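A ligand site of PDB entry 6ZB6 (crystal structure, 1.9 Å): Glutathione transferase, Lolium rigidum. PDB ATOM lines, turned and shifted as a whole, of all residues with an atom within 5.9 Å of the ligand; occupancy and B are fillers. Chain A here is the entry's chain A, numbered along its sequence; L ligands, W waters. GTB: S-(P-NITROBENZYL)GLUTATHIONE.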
ATOM      1  N   MET A  11       7.957  13.795  18.554  1.00  0.00           N
ATOM      2  CA  MET A  11       8.007  14.149  19.969  1.00  0.00           C
ATOM      3  C   MET A  11       8.290  12.950  20.866  1.00  0.00           C
ATOM      4  O   MET A  11       8.737  13.145  21.997  1.00  0.00           O
ATOM      5  CB  MET A  11       6.700  14.822  20.398  1.00  0.00           C
ATOM      6  CG  MET A  11       5.467  13.987  20.103  1.00  0.00           C
ATOM      7  SD  MET A  11       4.230  14.070  21.405  1.00  0.00           S
ATOM      8  CE  MET A  11       4.830  12.805  22.523  1.00  0.00           C
ATOM      9  N   SER A  12       8.014  11.733  20.407  1.00  0.00           N
ATOM     10  CA  SER A  12       8.284  10.555  21.223  1.00  0.00           C
ATOM     11  C   SER A  12       9.796  10.400  21.418  1.00  0.00           C
ATOM     12  O   SER A  12      10.561  10.484  20.458  1.00  0.00           O
ATOM     13  CB  SER A  12       7.698   9.310  20.558  1.00  0.00           C
ATOM     14  OG  SER A  12       8.258   8.121  21.081  1.00  0.00           O
ATOM     15  N   THR A  13      10.208  10.155  22.667  1.00  0.00           N
ATOM     16  CA  THR A  13      11.648  10.105  22.981  1.00  0.00           C
ATOM     17  C   THR A  13      12.410   9.154  22.063  1.00  0.00           C
ATOM     18  O   THR A  13      13.463   9.506  21.517  1.00  0.00           O
ATOM     19  CB  THR A  13      11.856   9.671  24.425  1.00  0.00           C
ATOM     20  OG1 THR A  13      10.980   8.577  24.725  1.00  0.00           O
ATOM     21  CG2 THR A  13      11.569  10.832  25.387  1.00  0.00           C
ATOM     22  N   ASN A  14      11.905   7.937  21.896  1.00  0.00           N
ATOM     23  CA  ASN A  14      12.702   6.960  21.171  1.00  0.00           C
ATOM     24  C   ASN A  14      12.601   7.145  19.665  1.00  0.00           C
ATOM     25  O   ASN A  14      13.489   6.677  18.939  1.00  0.00           O
ATOM     26  CB  ASN A  14      12.308   5.554  21.622  1.00  0.00           C
ATOM     27  CG  ASN A  14      12.644   5.314  23.091  1.00  0.00           C
ATOM     28  OD1 ASN A  14      13.809   5.362  23.485  1.00  0.00           O
ATOM     29  ND2 ASN A  14      11.619   5.110  23.908  1.00  0.00           N
ATOM     30  N   VAL A  15      11.581   7.856  19.176  1.00  0.00           N
ATOM     31  CA  VAL A  15      11.622   8.323  17.791  1.00  0.00           C
ATOM     32  C   VAL A  15      12.702   9.388  17.623  1.00  0.00           C
ATOM     33  O   VAL A  15      13.531   9.323  16.713  1.00  0.00           O
ATOM     34  CB  VAL A  15      10.244   8.857  17.361  1.00  0.00           C
ATOM     35  CG1 VAL A  15      10.353   9.540  16.008  1.00  0.00           C
ATOM     36  CG2 VAL A  15       9.212   7.728  17.339  1.00  0.00           C
ATOM     37  N   ARG A  17      15.293   9.873  19.232  1.00  0.00           N
ATOM     38  CA  ARG A  17      16.622   9.284  19.305  1.00  0.00           C
ATOM     39  C   ARG A  17      17.158   8.969  17.907  1.00  0.00           C
ATOM     40  O   ARG A  17      18.276   9.348  17.553  1.00  0.00           O
ATOM     41  CB  ARG A  17      16.586   8.019  20.187  1.00  0.00           C
ATOM     42  CG  ARG A  17      17.936   7.317  20.318  1.00  0.00           C
ATOM     43  CD  ARG A  17      17.821   5.876  20.806  1.00  0.00           C
ATOM     44  NE  ARG A  17      16.937   5.745  21.967  1.00  0.00           N
ATOM     45  CZ  ARG A  17      17.245   6.146  23.202  1.00  0.00           C
ATOM     46  NH1 ARG A  17      18.448   6.682  23.443  1.00  0.00           N
ATOM     47  NH2 ARG A  17      16.386   6.005  24.195  1.00  0.00           N
ATOM     48  N   PHE A  36      -1.892   8.255  18.257  1.00  0.00           N
ATOM     49  CA  PHE A  36      -2.063   7.475  19.469  1.00  0.00           C
ATOM     50  C   PHE A  36      -3.492   7.507  20.003  1.00  0.00           C
ATOM     51  O   PHE A  36      -3.869   6.602  20.755  1.00  0.00           O
ATOM     52  CB  PHE A  36      -1.092   7.955  20.540  1.00  0.00           C
ATOM     53  CG  PHE A  36       0.269   7.321  20.417  1.00  0.00           C
ATOM     54  CD1 PHE A  36       0.614   6.236  21.210  1.00  0.00           C
ATOM     55  CD2 PHE A  36       1.180   7.786  19.477  1.00  0.00           C
ATOM     56  CE1 PHE A  36       1.849   5.620  21.076  1.00  0.00           C
ATOM     57  CE2 PHE A  36       2.412   7.187  19.357  1.00  0.00           C
ATOM     58  CZ  PHE A  36       2.752   6.094  20.152  1.00  0.00           C
ATOM     59  N   HIS A  41      -0.546   2.649  16.854  1.00  0.00           N
ATOM     60  CA  HIS A  41       0.596   1.789  17.112  1.00  0.00           C
ATOM     61  C   HIS A  41       0.195   0.357  17.450  1.00  0.00           C
ATOM     62  O   HIS A  41       1.073  -0.519  17.459  1.00  0.00           O
ATOM     63  CB  HIS A  41       1.441   2.395  18.227  1.00  0.00           C
ATOM     64  CG  HIS A  41       0.697   2.582  19.513  1.00  0.00           C
ATOM     65  ND1 HIS A  41      -0.373   3.455  19.632  1.00  0.00           N
ATOM     66  CD2 HIS A  41       0.852   2.013  20.729  1.00  0.00           C
ATOM     67  CE1 HIS A  41      -0.838   3.398  20.868  1.00  0.00           C
ATOM     68  NE2 HIS A  41      -0.110   2.547  21.557  1.00  0.00           N
ATOM     69  N   LYS A  42      -1.082   0.089  17.724  1.00  0.00           N
ATOM     70  CA  LYS A  42      -1.582  -1.267  17.970  1.00  0.00           C
ATOM     71  C   LYS A  42      -2.382  -1.818  16.800  1.00  0.00           C
ATOM     72  O   LYS A  42      -3.030  -2.865  16.942  1.00  0.00           O
ATOM     73  CB  LYS A  42      -2.428  -1.306  19.251  1.00  0.00           C
ATOM     74  CG  LYS A  42      -1.730  -0.785  20.497  1.00  0.00           C
ATOM     75  CD  LYS A  42      -0.473  -1.603  20.792  1.00  0.00           C
ATOM     76  CE  LYS A  42       0.038  -1.358  22.203  1.00  0.00           C
ATOM     77  NZ  LYS A  42       1.371  -2.018  22.415  1.00  0.00           N
ATOM     78  N   ASN A  50       6.396  -3.272  13.924  1.00  0.00           N
ATOM     79  CA  ASN A  50       6.936  -3.529  15.256  1.00  0.00           C
ATOM     80  C   ASN A  50       5.950  -4.464  15.937  1.00  0.00           C
ATOM     81  O   ASN A  50       4.858  -4.022  16.325  1.00  0.00           O
ATOM     82  CB  ASN A  50       7.130  -2.254  16.079  1.00  0.00           C
ATOM     83  CG  ASN A  50       7.724  -2.537  17.466  1.00  0.00           C
ATOM     84  OD1 ASN A  50       7.629  -3.657  17.979  1.00  0.00           O
ATOM     85  ND2 ASN A  50       8.368  -1.544  18.047  1.00  0.00           N
ATOM     86  N   PHE A  52       5.667  -5.679  18.779  1.00  0.00           N
ATOM     87  CA  PHE A  52       5.305  -5.326  20.147  1.00  0.00           C
ATOM     88  C   PHE A  52       4.441  -4.075  20.219  1.00  0.00           C
ATOM     89  O   PHE A  52       4.066  -3.659  21.310  1.00  0.00           O
ATOM     90  CB  PHE A  52       6.590  -5.159  20.974  1.00  0.00           C
ATOM     91  CG  PHE A  52       7.410  -6.421  21.035  1.00  0.00           C
ATOM     92  CD1 PHE A  52       6.974  -7.515  21.795  1.00  0.00           C
ATOM     93  CD2 PHE A  52       8.586  -6.544  20.308  1.00  0.00           C
ATOM     94  CE1 PHE A  52       7.708  -8.689  21.840  1.00  0.00           C
ATOM     95  CE2 PHE A  52       9.329  -7.721  20.359  1.00  0.00           C
ATOM     96  CZ  PHE A  52       8.885  -8.798  21.119  1.00  0.00           C
ATOM     97  N   GLY A  53       4.100  -3.492  19.074  1.00  0.00           N
ATOM     98  CA  GLY A  53       3.139  -2.412  19.051  1.00  0.00           C
ATOM     99  C   GLY A  53       3.675  -1.171  19.731  1.00  0.00           C
ATOM    100  O   GLY A  53       2.995  -0.569  20.554  1.00  0.00           O
ATOM    101  N   GLN A  54       4.912  -0.794  19.389  1.00  0.00           N
ATOM    102  CA  GLN A  54       5.555   0.397  19.926  1.00  0.00           C
ATOM    103  C   GLN A  54       6.151   1.203  18.792  1.00  0.00           C
ATOM    104  O   GLN A  54       6.295   0.724  17.654  1.00  0.00           O
ATOM    105  CB  GLN A  54       6.664   0.031  20.936  1.00  0.00           C
ATOM    106  CG  GLN A  54       6.215  -0.720  22.178  1.00  0.00           C
ATOM    107  CD  GLN A  54       7.310  -0.775  23.238  1.00  0.00           C
ATOM    108  OE1 GLN A  54       8.432  -1.205  22.959  1.00  0.00           O
ATOM    109  NE2 GLN A  54       7.000  -0.305  24.445  1.00  0.00           N
ATOM    110  N   ILE A  55       6.518   2.448  19.098  1.00  0.00           N
ATOM    111  CA  ILE A  55       7.257   3.285  18.157  1.00  0.00           C
ATOM    112  C   ILE A  55       8.619   3.563  18.766  1.00  0.00           C
ATOM    113  O   ILE A  55       8.744   3.598  20.004  1.00  0.00           O
ATOM    114  CB  ILE A  55       6.492   4.578  17.834  1.00  0.00           C
ATOM    115  CG1 ILE A  55       6.159   5.347  19.118  1.00  0.00           C
ATOM    116  CG2 ILE A  55       5.232   4.288  17.035  1.00  0.00           C
ATOM    117  CD1 ILE A  55       5.903   6.808  18.878  1.00  0.00           C
ATOM    118  N   PRO A  56       9.665   3.782  17.963  1.00  0.00           N
ATOM    119  CA  PRO A  56       9.622   3.854  16.498  1.00  0.00           C
ATOM    120  C   PRO A  56       9.558   2.491  15.826  1.00  0.00           C
ATOM    121  O   PRO A  56       9.912   1.484  16.446  1.00  0.00           O
ATOM    122  CB  PRO A  56      10.967   4.499  16.156  1.00  0.00           C
ATOM    123  CG  PRO A  56      11.885   3.966  17.207  1.00  0.00           C
ATOM    124  CD  PRO A  56      11.023   4.002  18.476  1.00  0.00           C
ATOM    125  N   PHE A  66      12.934  -2.273  14.238  1.00  0.00           N
ATOM    126  CA  PHE A  66      12.380  -1.573  15.384  1.00  0.00           C
ATOM    127  C   PHE A  66      13.446  -1.616  16.473  1.00  0.00           C
ATOM    128  O   PHE A  66      14.546  -2.135  16.255  1.00  0.00           O
ATOM    129  CB  PHE A  66      11.031  -2.170  15.811  1.00  0.00           C
ATOM    130  CG  PHE A  66      11.106  -3.610  16.246  1.00  0.00           C
ATOM    131  CD1 PHE A  66      11.035  -4.641  15.318  1.00  0.00           C
ATOM    132  CD2 PHE A  66      11.209  -3.932  17.590  1.00  0.00           C
ATOM    133  CE1 PHE A  66      11.100  -5.977  15.730  1.00  0.00           C
ATOM    134  CE2 PHE A  66      11.279  -5.247  18.005  1.00  0.00           C
ATOM    135  CZ  PHE A  66      11.207  -6.278  17.077  1.00  0.00           C
ATOM    136  N   GLU A  67      13.106  -1.038  17.633  1.00  0.00           N
ATOM    137  CA  GLU A  67      14.042  -0.754  18.728  1.00  0.00           C
ATOM    138  C   GLU A  67      14.972   0.380  18.336  1.00  0.00           C
ATOM    139  O   GLU A  67      15.805   0.246  17.440  1.00  0.00           O
ATOM    140  CB  GLU A  67      14.826  -2.001  19.174  1.00  0.00           C
ATOM    141  CG  GLU A  67      14.068  -2.874  20.161  1.00  0.00           C
ATOM    142  CD  GLU A  67      13.836  -2.218  21.532  1.00  0.00           C
ATOM    143  OE1 GLU A  67      14.536  -1.232  21.885  1.00  0.00           O
ATOM    144  OE2 GLU A  67      12.935  -2.700  22.250  1.00  0.00           O
ATOM    145  N   SER A  68      14.823   1.522  19.017  1.00  0.00           N
ATOM    146  CA  SER A  68      15.458   2.754  18.571  1.00  0.00           C
ATOM    147  C   SER A  68      16.980   2.648  18.484  1.00  0.00           C
ATOM    148  O   SER A  68      17.588   3.174  17.555  1.00  0.00           O
ATOM    149  CB  SER A  68      15.032   3.901  19.506  1.00  0.00           C
ATOM    150  OG  SER A  68      15.420   3.631  20.831  1.00  0.00           O
ATOM    151  N   ARG A  69      17.632   1.979  19.448  1.00  0.00           N
ATOM    152  CA  ARG A  69      19.087   1.917  19.390  1.00  0.00           C
ATOM    153  C   ARG A  69      19.570   1.043  18.238  1.00  0.00           C
ATOM    154  O   ARG A  69      20.617   1.329  17.650  1.00  0.00           O
ATOM    155  CB  ARG A  69      19.672   1.420  20.700  1.00  0.00           C
ATOM    156  CG  ARG A  69      19.503   2.429  21.852  1.00  0.00           C
ATOM    157  CD  ARG A  69      19.988   1.822  23.158  1.00  0.00           C
ATOM    158  NE  ARG A  69      19.710   2.703  24.311  1.00  0.00           N
ATOM    159  CZ  ARG A  69      18.536   2.816  24.920  1.00  0.00           C
ATOM    160  NH1 ARG A  69      17.499   2.132  24.495  1.00  0.00           N
ATOM    161  NH2 ARG A  69      18.401   3.638  25.965  1.00  0.00           N
ATOM    162  N   TYR A 118       8.291  10.595  33.315  1.00  0.00           N
ATOM    163  CA  TYR A 118       6.966   9.973  33.295  1.00  0.00           C
ATOM    164  C   TYR A 118       6.046  10.618  34.321  1.00  0.00           C
ATOM    165  O   TYR A 118       4.918  11.013  34.007  1.00  0.00           O
ATOM    166  CB  TYR A 118       7.072   8.473  33.566  1.00  0.00           C
ATOM    167  CG  TYR A 118       7.278   7.643  32.325  1.00  0.00           C
ATOM    168  CD1 TYR A 118       6.192   7.192  31.577  1.00  0.00           C
ATOM    169  CD2 TYR A 118       8.553   7.313  31.896  1.00  0.00           C
ATOM    170  CE1 TYR A 118       6.374   6.425  30.438  1.00  0.00           C
ATOM    171  CE2 TYR A 118       8.751   6.547  30.753  1.00  0.00           C
ATOM    172  CZ  TYR A 118       7.654   6.109  30.029  1.00  0.00           C
ATOM    173  OH  TYR A 118       7.860   5.354  28.897  1.00  0.00           O
ATOM    174  N   PHE A 122       4.790  13.027  31.286  1.00  0.00           N
ATOM    175  CA  PHE A 122       3.978  12.132  30.468  1.00  0.00           C
ATOM    176  C   PHE A 122       2.667  11.783  31.167  1.00  0.00           C
ATOM    177  O   PHE A 122       1.587  11.919  30.581  1.00  0.00           O
ATOM    178  CB  PHE A 122       4.750  10.842  30.146  1.00  0.00           C
ATOM    179  CG  PHE A 122       5.976  11.039  29.274  1.00  0.00           C
ATOM    180  CD1 PHE A 122       6.133  12.168  28.477  1.00  0.00           C
ATOM    181  CD2 PHE A 122       6.977  10.062  29.237  1.00  0.00           C
ATOM    182  CE1 PHE A 122       7.261  12.331  27.673  1.00  0.00           C
ATOM    183  CE2 PHE A 122       8.109  10.213  28.441  1.00  0.00           C
ATOM    184  CZ  PHE A 122       8.249  11.354  27.654  1.00  0.00           C
ATOM    185  N   ASN A 123       2.736  11.326  32.416  1.00  0.00           N
ATOM    186  CA  ASN A 123       1.530  10.861  33.106  1.00  0.00           C
ATOM    187  C   ASN A 123       0.467  11.941  33.230  1.00  0.00           C
ATOM    188  O   ASN A 123      -0.684  11.689  32.840  1.00  0.00           O
ATOM    189  CB  ASN A 123       1.904  10.271  34.471  1.00  0.00           C
ATOM    190  CG  ASN A 123       2.429   8.848  34.380  1.00  0.00           C
ATOM    191  OD1 ASN A 123       2.776   8.368  33.296  1.00  0.00           O
ATOM    192  ND2 ASN A 123       2.499   8.176  35.521  1.00  0.00           N
ATOM    193  N   MET A 126      -0.134  13.612  29.158  1.00  0.00           N
ATOM    194  CA  MET A 126      -0.524  12.684  28.100  1.00  0.00           C
ATOM    195  C   MET A 126      -1.603  11.715  28.553  1.00  0.00           C
ATOM    196  O   MET A 126      -2.560  11.452  27.807  1.00  0.00           O
ATOM    197  CB  MET A 126       0.697  11.902  27.612  1.00  0.00           C
ATOM    198  CG  MET A 126       1.717  12.758  26.878  1.00  0.00           C
ATOM    199  SD  MET A 126       0.994  14.208  26.083  1.00  0.00           S
ATOM    200  CE  MET A 126       0.635  13.547  24.463  1.00  0.00           C
ATOM    201  N   ARG A 127      -1.483  11.162  29.755  1.00  0.00           N
ATOM    202  CA  ARG A 127      -2.391  10.114  30.212  1.00  0.00           C
ATOM    203  C   ARG A 127      -3.406  10.600  31.238  1.00  0.00           C
ATOM    204  O   ARG A 127      -4.242   9.803  31.685  1.00  0.00           O
ATOM    205  CB  ARG A 127      -1.590   8.941  30.800  1.00  0.00           C
ATOM    206  CG  ARG A 127      -0.769   8.199  29.776  1.00  0.00           C
ATOM    207  CD  ARG A 127      -0.559   6.752  30.196  1.00  0.00           C
ATOM    208  NE  ARG A 127       0.852   6.448  30.370  1.00  0.00           N
ATOM    209  CZ  ARG A 127       1.419   6.143  31.530  1.00  0.00           C
ATOM    210  NH1 ARG A 127       0.680   6.107  32.640  1.00  0.00           N
ATOM    211  NH2 ARG A 127       2.719   5.872  31.605  1.00  0.00           N
ATOM    212  N   TYR A 175      15.502  11.682  26.553  1.00  0.00           N
ATOM    213  CA  TYR A 175      14.828  11.729  27.850  1.00  0.00           C
ATOM    214  C   TYR A 175      15.322  12.896  28.697  1.00  0.00           C
ATOM    215  O   TYR A 175      14.527  13.510  29.418  1.00  0.00           O
ATOM    216  CB  TYR A 175      14.998  10.430  28.620  1.00  0.00           C
ATOM    217  CG  TYR A 175      14.152   9.282  28.104  1.00  0.00           C
ATOM    218  CD1 TYR A 175      14.569   8.523  27.032  1.00  0.00           C
ATOM    219  CD2 TYR A 175      12.938   8.949  28.708  1.00  0.00           C
ATOM    220  CE1 TYR A 175      13.812   7.475  26.548  1.00  0.00           C
ATOM    221  CE2 TYR A 175      12.164   7.893  28.244  1.00  0.00           C
ATOM    222  CZ  TYR A 175      12.604   7.151  27.149  1.00  0.00           C
ATOM    223  OH  TYR A 175      11.879   6.086  26.664  1.00  0.00           O
HETATM  224  N1  GTB L   1      12.986  -0.056  23.698  1.00  0.00           N
HETATM  225  CA1 GTB L   1      12.075   0.599  22.771  1.00  0.00           C
HETATM  226  C1  GTB L   1      12.866   1.512  21.829  1.00  0.00           C
HETATM  227  O11 GTB L   1      13.865   2.158  22.254  1.00  0.00           O
HETATM  228  O12 GTB L   1      12.536   1.629  20.616  1.00  0.00           O
HETATM  229  CB1 GTB L   1      11.053   1.398  23.601  1.00  0.00           C
HETATM  230  CG1 GTB L   1      10.109   2.109  22.640  1.00  0.00           C
HETATM  231  CD1 GTB L   1       8.933   2.735  23.384  1.00  0.00           C
HETATM  232  OE1 GTB L   1       8.829   2.657  24.566  1.00  0.00           O
HETATM  233  N2  GTB L   1       7.951   3.443  22.604  1.00  0.00           N
HETATM  234  CA2 GTB L   1       6.832   4.033  23.322  1.00  0.00           C
HETATM  235  C2  GTB L   1       5.557   3.334  22.883  1.00  0.00           C
HETATM  236  O2  GTB L   1       5.352   3.074  21.736  1.00  0.00           O
HETATM  237  CB2 GTB L   1       6.764   5.525  23.012  1.00  0.00           C
HETATM  238  SG2 GTB L   1       8.258   6.336  23.702  1.00  0.00           S
HETATM  239  N3  GTB L   1       4.594   2.945  23.881  1.00  0.00           N
HETATM  240  CA3 GTB L   1       3.374   2.291  23.459  1.00  0.00           C
HETATM  241  C3  GTB L   1       3.238   0.937  24.150  1.00  0.00           C
HETATM  242  O31 GTB L   1       2.102   0.390  24.224  1.00  0.00           O
HETATM  243  O32 GTB L   1       4.248   0.357  24.627  1.00  0.00           O
HETATM  244  C'  GTB L   1       8.179   6.245  25.513  1.00  0.00           C
HETATM  245  C1' GTB L   1       6.920   6.971  25.974  1.00  0.00           C
HETATM  246  C2' GTB L   1       5.906   6.260  26.608  1.00  0.00           C
HETATM  247  C3' GTB L   1       4.763   6.914  27.030  1.00  0.00           C
HETATM  248  C4' GTB L   1       4.628   8.283  26.826  1.00  0.00           C
HETATM  249  N41 GTB L   1       3.416   8.968  27.272  1.00  0.00           N
HETATM  250  O41 GTB L   1       2.426   8.298  28.020  1.00  0.00           O
HETATM  251  O42 GTB L   1       3.271  10.105  27.001  1.00  0.00           O
HETATM  252  C5' GTB L   1       5.645   8.984  26.200  1.00  0.00           C
HETATM  253  C6' GTB L   1       6.793   8.338  25.775  1.00  0.00           C
HETATM  254  O   HOH W   1      -0.029   1.952  24.266  1.00  0.00           O
HETATM  255  O   HOH W   2      10.897  -1.803  24.710  1.00  0.00           O
HETATM  256  O   HOH W   3      10.193   2.367  26.884  1.00  0.00           O
HETATM  257  O   HOH W   4      16.817   0.428  21.826  1.00  0.00           O
HETATM  258  O   HOH W   5      10.904   0.282  18.924  1.00  0.00           O
HETATM  259  O   HOH W   6       3.313  -2.602  25.247  1.00  0.00           O
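The guanidinium group (NE) of Arg 17 sits at hydrogen-bond distance from the side-chain hydroxyl (OG) of Ser 68, 2.8 Å away. ND2 of Asn 50 lies within hydrogen-bond range of O of Gln 54 (3.1 Å). The backbone carbonyl oxygen of Phe 52 lies within hydrogen-bond range of the side-chain amino group of Lys 42 (3.3 Å). The backbone carbonyl oxygen (O) of Tyr 118 lies within hydrogen-bond range of the backbone NH (N) of Asn 123, at 2.7 Å. The backbone NH of Arg 127 lies within hydrogen-bond range of the backbone carbonyl oxygen of Phe 122 (3.3 Å). NH2 of Arg 127 sits at hydrogen-bond distance from OD1 of Asn 123 (3.0 Å). The side-chain amide nitrogen (ND2) of Asn 14 sits at hydrogen-bond distance from the side-chain hydroxyl (OH) of Tyr 175 (2.9 Å). NH2 of Arg 17 lies within hydrogen-bond range of OD1 of Asn 14 (2.7 Å).
The backbone NH (N) of Ser 68 sits at hydrogen-bond distance from an oxygen (O12) of the ligand, at 2.8 Å. The side-chain hydroxyl (OG) of Ser 68 lies within hydrogen-bond range of an oxygen (O11) of the ligand (2.6 Å). The side-chain carboxylate (OE1) of Glu 67 is in salt-bridge range of a nitrogen (N1) of the ligand (2.7 Å). An oxygen (O2) of the ligand sits at hydrogen-bond distance from the backbone NH of Ile 55 (3.0 Å). The backbone carbonyl oxygen (O) of Ile 55 sits at hydrogen-bond distance from a nitrogen (N2) of the ligand, 2.7 Å away. The side-chain amide nitrogen (NE2) of Gln 54 lies within hydrogen-bond range of an oxygen (O32) of the ligand. NZ of Lys 42 lies within salt-bridge range of O31 of the ligand (3.1 Å). OG of Ser 12 sits close to SG2 of the ligand, at 3.2 Å. An oxygen (O41) of the ligand lies within hydrogen-bond range of the guanidinium group of Arg 127. The side-chain amide oxygen (OD1) of Asn 14 lies close to an oxygen (O11) of the ligand (3.4 Å). A sulfur (SG2) of the ligand sits close to the side-chain hydroxyl (OG1) of Thr 13 (3.7 Å).
Water W1 bridges O31 of the ligand and NE2 of His 41. Water W5 lies within hydrogen-bond range of O12 of the ligand, N of Glu 67, O of Pro 56 and ND2 of Asn 50. Water W2 lies within hydrogen-bond range of a nitrogen (N1) of the ligand (2.9 Å), the side-chain amide oxygen (OE1) of Gln 54 (3.1 Å) and the side-chain carboxylate (OE2) of Glu 67 (3.3 Å). Water W6 bridges an oxygen (O32) of the ligand and the side-chain amino group (NZ) of Lys 42. Water W4 lies within hydrogen-bond range of OE1 of Glu 67 (2.8 Å), N of Arg 69 (3.0 Å) and O11 of the ligand (3.4 Å).
His 41 touches the ligand. O of Gly 53 touches O31 of the ligand, 3.9 Å away. CD of Pro 56 touches O12 of the ligand, at 3.5 Å. Tyr 118 touches the ligand. CD2 of Phe 122 touches C5' of the ligand, 3.5 Å away. Met 126 touches the ligand. Tyr 175 touches the ligand. 16 residues have an atom within 4 Å of the ligand: Ser 12, Thr 13, Asn 14, His 41, Lys 42, Gly 53, Gln 54, Ile 55, Pro 56, Glu 67, Ser 68, Tyr 118, Phe 122, Met 126, Arg 127 and Tyr 175. The nearest printed residue that does not touch the ligand is Arg 69 (4.3 Å).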
